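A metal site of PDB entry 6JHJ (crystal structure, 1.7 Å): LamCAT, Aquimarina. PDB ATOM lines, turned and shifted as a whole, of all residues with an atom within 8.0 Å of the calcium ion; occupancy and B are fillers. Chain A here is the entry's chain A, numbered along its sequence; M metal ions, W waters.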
ATOM      1  N   ASP A  10     -15.792  -3.257   1.402  1.00  0.00           N
ATOM      2  CA  ASP A  10     -14.534  -4.060   1.499  1.00  0.00           C
ATOM      3  C   ASP A  10     -14.562  -4.676   2.884  1.00  0.00           C
ATOM      4  O   ASP A  10     -14.582  -3.932   3.871  1.00  0.00           O
ATOM      5  CB  ASP A  10     -13.297  -3.224   1.315  1.00  0.00           C
ATOM      6  CG  ASP A  10     -12.069  -4.046   1.012  1.00  0.00           C
ATOM      7  OD1 ASP A  10     -12.119  -5.282   1.239  1.00  0.00           O
ATOM      8  OD2 ASP A  10     -11.062  -3.470   0.522  1.00  0.00           O
ATOM      9  N   GLU A  11     -14.619  -5.990   2.960  1.00  0.00           N
ATOM     10  CA  GLU A  11     -14.634  -6.716   4.234  1.00  0.00           C
ATOM     11  C   GLU A  11     -13.243  -7.148   4.597  1.00  0.00           C
ATOM     12  O   GLU A  11     -13.066  -7.704   5.722  1.00  0.00           O
ATOM     13  CB  GLU A  11     -15.511  -7.958   4.185  1.00  0.00           C
ATOM     14  CG  GLU A  11     -16.943  -7.697   3.757  1.00  0.00           C
ATOM     15  CD  GLU A  11     -17.661  -6.833   4.771  1.00  0.00           C
ATOM     16  OE1 GLU A  11     -17.557  -7.143   6.007  1.00  0.00           O
ATOM     17  OE2 GLU A  11     -18.372  -5.867   4.364  1.00  0.00           O
ATOM     18  N   PHE A  12     -12.282  -6.903   3.701  1.00  0.00           N
ATOM     19  CA  PHE A  12     -10.857  -7.214   3.921  1.00  0.00           C
ATOM     20  C   PHE A  12     -10.640  -8.700   4.146  1.00  0.00           C
ATOM     21  O   PHE A  12      -9.664  -9.099   4.774  1.00  0.00           O
ATOM     22  CB  PHE A  12     -10.285  -6.402   5.056  1.00  0.00           C
ATOM     23  CG  PHE A  12     -10.410  -4.947   4.851  1.00  0.00           C
ATOM     24  CD1 PHE A  12      -9.676  -4.326   3.827  1.00  0.00           C
ATOM     25  CD2 PHE A  12     -11.261  -4.185   5.609  1.00  0.00           C
ATOM     26  CE1 PHE A  12      -9.813  -2.952   3.574  1.00  0.00           C
ATOM     27  CE2 PHE A  12     -11.415  -2.823   5.344  1.00  0.00           C
ATOM     28  CZ  PHE A  12     -10.680  -2.218   4.337  1.00  0.00           C
ATOM     29  N   THR A  13     -11.585  -9.494   3.732  1.00  0.00           N
ATOM     30  CA  THR A  13     -11.535 -10.914   4.086  1.00  0.00           C
ATOM     31  C   THR A  13     -10.475 -11.603   3.220  1.00  0.00           C
ATOM     32  O   THR A  13      -9.688 -12.384   3.773  1.00  0.00           O
ATOM     33  CB  THR A  13     -12.903 -11.617   3.996  1.00  0.00           C
ATOM     34  OG1 THR A  13     -13.456 -11.248   2.775  1.00  0.00           O
ATOM     35  CG2 THR A  13     -13.795 -11.143   5.026  1.00  0.00           C
ATOM     36  N   ASN A  14     -10.394 -11.259   1.933  1.00  0.00           N
ATOM     37  CA  ASN A  14      -9.326 -11.764   1.073  1.00  0.00           C
ATOM     38  C   ASN A  14      -8.414 -10.630   0.545  1.00  0.00           C
ATOM     39  O   ASN A  14      -8.448 -10.297  -0.630  1.00  0.00           O
ATOM     40  CB  ASN A  14      -9.984 -12.610  -0.001  1.00  0.00           C
ATOM     41  CG  ASN A  14     -10.819 -13.775   0.629  1.00  0.00           C
ATOM     42  OD1 ASN A  14     -12.041 -13.854   0.478  1.00  0.00           O
ATOM     43  ND2 ASN A  14     -10.154 -14.633   1.399  1.00  0.00           N
ATOM     44  N   VAL A  46      -3.207  -6.907   5.994  1.00  0.00           N
ATOM     45  CA  VAL A  46      -4.484  -7.539   6.423  1.00  0.00           C
ATOM     46  C   VAL A  46      -4.166  -8.641   7.375  1.00  0.00           C
ATOM     47  O   VAL A  46      -3.252  -9.412   7.077  1.00  0.00           O
ATOM     48  CB  VAL A  46      -5.340  -8.044   5.285  1.00  0.00           C
ATOM     49  CG1 VAL A  46      -6.516  -8.878   5.739  1.00  0.00           C
ATOM     50  CG2 VAL A  46      -5.860  -6.915   4.420  1.00  0.00           C
ATOM     51  N   GLU A  47      -4.906  -8.710   8.504  1.00  0.00           N
ATOM     52  CA  GLU A  47      -4.721  -9.807   9.484  1.00  0.00           C
ATOM     53  C   GLU A  47      -6.118 -10.259   9.898  1.00  0.00           C
ATOM     54  O   GLU A  47      -6.885  -9.479  10.460  1.00  0.00           O
ATOM     55  CB  GLU A  47      -3.998  -9.323  10.705  1.00  0.00           C
ATOM     56  CG  GLU A  47      -2.583  -8.839  10.479  1.00  0.00           C
ATOM     57  CD  GLU A  47      -1.933  -8.398  11.776  1.00  0.00           C
ATOM     58  OE1 GLU A  47      -2.552  -8.550  12.871  1.00  0.00           O
ATOM     59  OE2 GLU A  47      -0.828  -7.826  11.686  1.00  0.00           O
ATOM     60  N   ASN A  48      -6.408 -11.518   9.629  1.00  0.00           N
ATOM     61  CA  ASN A  48      -7.655 -12.133  10.028  1.00  0.00           C
ATOM     62  C   ASN A  48      -8.886 -11.298   9.675  1.00  0.00           C
ATOM     63  O   ASN A  48      -9.707 -10.995  10.550  1.00  0.00           O
ATOM     64  CB  ASN A  48      -7.658 -12.421  11.542  1.00  0.00           C
ATOM     65  CG  ASN A  48      -8.688 -13.483  11.922  1.00  0.00           C
ATOM     66  OD1 ASN A  48      -9.005 -14.386  11.132  1.00  0.00           O
ATOM     67  ND2 ASN A  48      -9.218 -13.376  13.129  1.00  0.00           N
ATOM     68  N   GLY A  49      -8.978 -10.866   8.433  1.00  0.00           N
ATOM     69  CA  GLY A  49     -10.240 -10.236   7.993  1.00  0.00           C
ATOM     70  C   GLY A  49     -10.294  -8.758   8.430  1.00  0.00           C
ATOM     71  O   GLY A  49     -11.363  -8.180   8.384  1.00  0.00           O
ATOM     72  N   ASN A  50      -9.172  -8.156   8.842  1.00  0.00           N
ATOM     73  CA  ASN A  50      -9.123  -6.760   9.176  1.00  0.00           C
ATOM     74  C   ASN A  50      -7.996  -6.062   8.439  1.00  0.00           C
ATOM     75  O   ASN A  50      -6.909  -6.545   8.389  1.00  0.00           O
ATOM     76  CB  ASN A  50      -8.789  -6.528  10.669  1.00  0.00           C
ATOM     77  CG  ASN A  50      -9.941  -6.796  11.588  1.00  0.00           C
ATOM     78  OD1 ASN A  50     -10.446  -5.902  12.211  1.00  0.00           O
ATOM     79  ND2 ASN A  50     -10.339  -8.027  11.696  1.00  0.00           N
ATOM     80  N   LEU A  51      -8.254  -4.868   7.922  1.00  0.00           N
ATOM     81  CA  LEU A  51      -7.211  -3.988   7.442  1.00  0.00           C
ATOM     82  C   LEU A  51      -6.432  -3.545   8.642  1.00  0.00           C
ATOM     83  O   LEU A  51      -7.024  -3.195   9.685  1.00  0.00           O
ATOM     84  CB  LEU A  51      -7.860  -2.783   6.837  1.00  0.00           C
ATOM     85  CG  LEU A  51      -6.918  -1.655   6.435  1.00  0.00           C
ATOM     86  CD1 LEU A  51      -5.995  -2.002   5.270  1.00  0.00           C
ATOM     87  CD2 LEU A  51      -7.797  -0.440   6.099  1.00  0.00           C
ATOM     88  N   ARG A  86     -16.224  -0.128  10.720  1.00  0.00           N
ATOM     89  CA  ARG A  86     -16.001  -0.614  12.070  1.00  0.00           C
ATOM     90  C   ARG A  86     -14.512  -0.512  12.342  1.00  0.00           C
ATOM     91  O   ARG A  86     -13.731  -1.137  11.638  1.00  0.00           O
ATOM     92  CB  ARG A  86     -16.460  -2.065  12.179  1.00  0.00           C
ATOM     93  CG  ARG A  86     -16.413  -2.569  13.587  1.00  0.00           C
ATOM     94  CD  ARG A  86     -17.277  -3.796  13.753  1.00  0.00           C
ATOM     95  NE  ARG A  86     -17.230  -4.246  15.108  1.00  0.00           N
ATOM     96  CZ  ARG A  86     -16.548  -5.273  15.558  1.00  0.00           C
ATOM     97  NH1 ARG A  86     -15.787  -6.020  14.796  1.00  0.00           N
ATOM     98  NH2 ARG A  86     -16.662  -5.573  16.846  1.00  0.00           N
ATOM     99  N   TYR A 157     -13.271  -1.703  19.069  1.00  0.00           N
ATOM    100  CA  TYR A 157     -14.034  -1.481  17.832  1.00  0.00           C
ATOM    101  C   TYR A 157     -15.272  -0.714  18.107  1.00  0.00           C
ATOM    102  O   TYR A 157     -16.037  -1.029  19.058  1.00  0.00           O
ATOM    103  CB  TYR A 157     -14.471  -2.767  17.182  1.00  0.00           C
ATOM    104  CG  TYR A 157     -13.394  -3.591  16.547  1.00  0.00           C
ATOM    105  CD1 TYR A 157     -12.841  -3.242  15.330  1.00  0.00           C
ATOM    106  CD2 TYR A 157     -12.909  -4.736  17.198  1.00  0.00           C
ATOM    107  CE1 TYR A 157     -11.855  -4.021  14.735  1.00  0.00           C
ATOM    108  CE2 TYR A 157     -11.939  -5.515  16.609  1.00  0.00           C
ATOM    109  CZ  TYR A 157     -11.432  -5.172  15.390  1.00  0.00           C
ATOM    110  OH  TYR A 157     -10.482  -6.000  14.792  1.00  0.00           O
ATOM    111  N   VAL A 225      -9.405  -1.893  10.811  1.00  0.00           N
ATOM    112  CA  VAL A 225     -10.688  -1.614  10.176  1.00  0.00           C
ATOM    113  C   VAL A 225     -11.311  -2.954   9.732  1.00  0.00           C
ATOM    114  O   VAL A 225     -10.732  -3.628   8.892  1.00  0.00           O
ATOM    115  CB  VAL A 225     -10.524  -0.676   8.986  1.00  0.00           C
ATOM    116  CG1 VAL A 225     -11.871  -0.343   8.385  1.00  0.00           C
ATOM    117  CG2 VAL A 225      -9.813   0.594   9.411  1.00  0.00           C
ATOM    118  N   ASP A 226     -12.406  -3.386  10.364  1.00  0.00           N
ATOM    119  CA  ASP A 226     -13.031  -4.630  10.110  1.00  0.00           C
ATOM    120  C   ASP A 226     -13.706  -4.605   8.766  1.00  0.00           C
ATOM    121  O   ASP A 226     -13.706  -5.589   8.061  1.00  0.00           O
ATOM    122  CB  ASP A 226     -14.003  -4.906  11.254  1.00  0.00           C
ATOM    123  CG  ASP A 226     -14.572  -6.353  11.255  1.00  0.00           C
ATOM    124  OD1 ASP A 226     -14.171  -7.241  10.495  1.00  0.00           O
ATOM    125  OD2 ASP A 226     -15.510  -6.501  12.025  1.00  0.00           O
ATOM    126  N   TYR A 227     -14.309  -3.488   8.406  1.00  0.00           N
ATOM    127  CA  TYR A 227     -14.949  -3.324   7.097  1.00  0.00           C
ATOM    128  C   TYR A 227     -15.261  -1.875   6.811  1.00  0.00           C
ATOM    129  O   TYR A 227     -15.326  -1.040   7.745  1.00  0.00           O
ATOM    130  CB  TYR A 227     -16.260  -4.096   7.060  1.00  0.00           C
ATOM    131  CG  TYR A 227     -17.208  -3.749   8.152  1.00  0.00           C
ATOM    132  CD1 TYR A 227     -18.014  -2.640   8.033  1.00  0.00           C
ATOM    133  CD2 TYR A 227     -17.420  -4.621   9.253  1.00  0.00           C
ATOM    134  CE1 TYR A 227     -18.964  -2.323   8.988  1.00  0.00           C
ATOM    135  CE2 TYR A 227     -18.371  -4.304  10.208  1.00  0.00           C
ATOM    136  CZ  TYR A 227     -19.118  -3.142  10.055  1.00  0.00           C
ATOM    137  OH  TYR A 227     -20.048  -2.762  10.945  1.00  0.00           O
ATOM    138  N   VAL A 228     -15.559  -1.610   5.544  1.00  0.00           N
ATOM    139  CA  VAL A 228     -16.081  -0.338   5.048  1.00  0.00           C
ATOM    140  C   VAL A 228     -17.296  -0.737   4.151  1.00  0.00           C
ATOM    141  O   VAL A 228     -17.156  -1.641   3.355  1.00  0.00           O
ATOM    142  CB  VAL A 228     -15.083   0.468   4.226  1.00  0.00           C
ATOM    143  CG1 VAL A 228     -15.675   1.808   3.910  1.00  0.00           C
ATOM    144  CG2 VAL A 228     -13.831   0.744   5.068  1.00  0.00           C
ATOM    145  N   ARG A 229     -18.421  -0.100   4.300  1.00  0.00           N
ATOM    146  CA  ARG A 229     -19.630  -0.433   3.537  1.00  0.00           C
ATOM    147  C   ARG A 229     -20.297   0.821   3.085  1.00  0.00           C
ATOM    148  O   ARG A 229     -20.380   1.794   3.830  1.00  0.00           O
ATOM    149  CB  ARG A 229     -20.615  -1.262   4.373  1.00  0.00           C
ATOM    150  CG  ARG A 229     -20.103  -2.661   4.718  1.00  0.00           C
ATOM    151  CD  ARG A 229     -20.821  -3.305   5.907  1.00  0.00           C
ATOM    152  NE  ARG A 229     -20.166  -4.597   6.240  1.00  0.00           N
ATOM    153  CZ  ARG A 229     -20.471  -5.296   7.318  1.00  0.00           C
ATOM    154  NH1 ARG A 229     -21.446  -4.895   8.149  1.00  0.00           N
ATOM    155  NH2 ARG A 229     -19.807  -6.409   7.558  1.00  0.00           N
HETATM  156 CA    CA M   1     -13.520  -7.822   8.007  1.00  0.00          CA
HETATM  157  O   HOH W   1     -15.975  -7.991   7.740  1.00  0.00           O
HETATM  158  O   HOH W   2     -14.220  -9.956   9.109  1.00  0.00           O
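The side-chain carboxylate (OD2) of Asp 226 lies within salt-bridge range of the guanidinium group (NH1) of Arg 86 (2.8 Å).
The guanidinium group (NH2) of Arg 229 is in salt-bridge range of the side-chain carboxylate (OE1) of Glu 11 (2.8 Å).
The calcium ion is bound by O of Gly 49 (2.2 Å), O of Asp 226 (2.2 Å), O of Glu 11 (2.3 Å), water W1 (2.5 Å), water W2 (2.5 Å) and OD1 of Asp 226 (2.6 Å).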
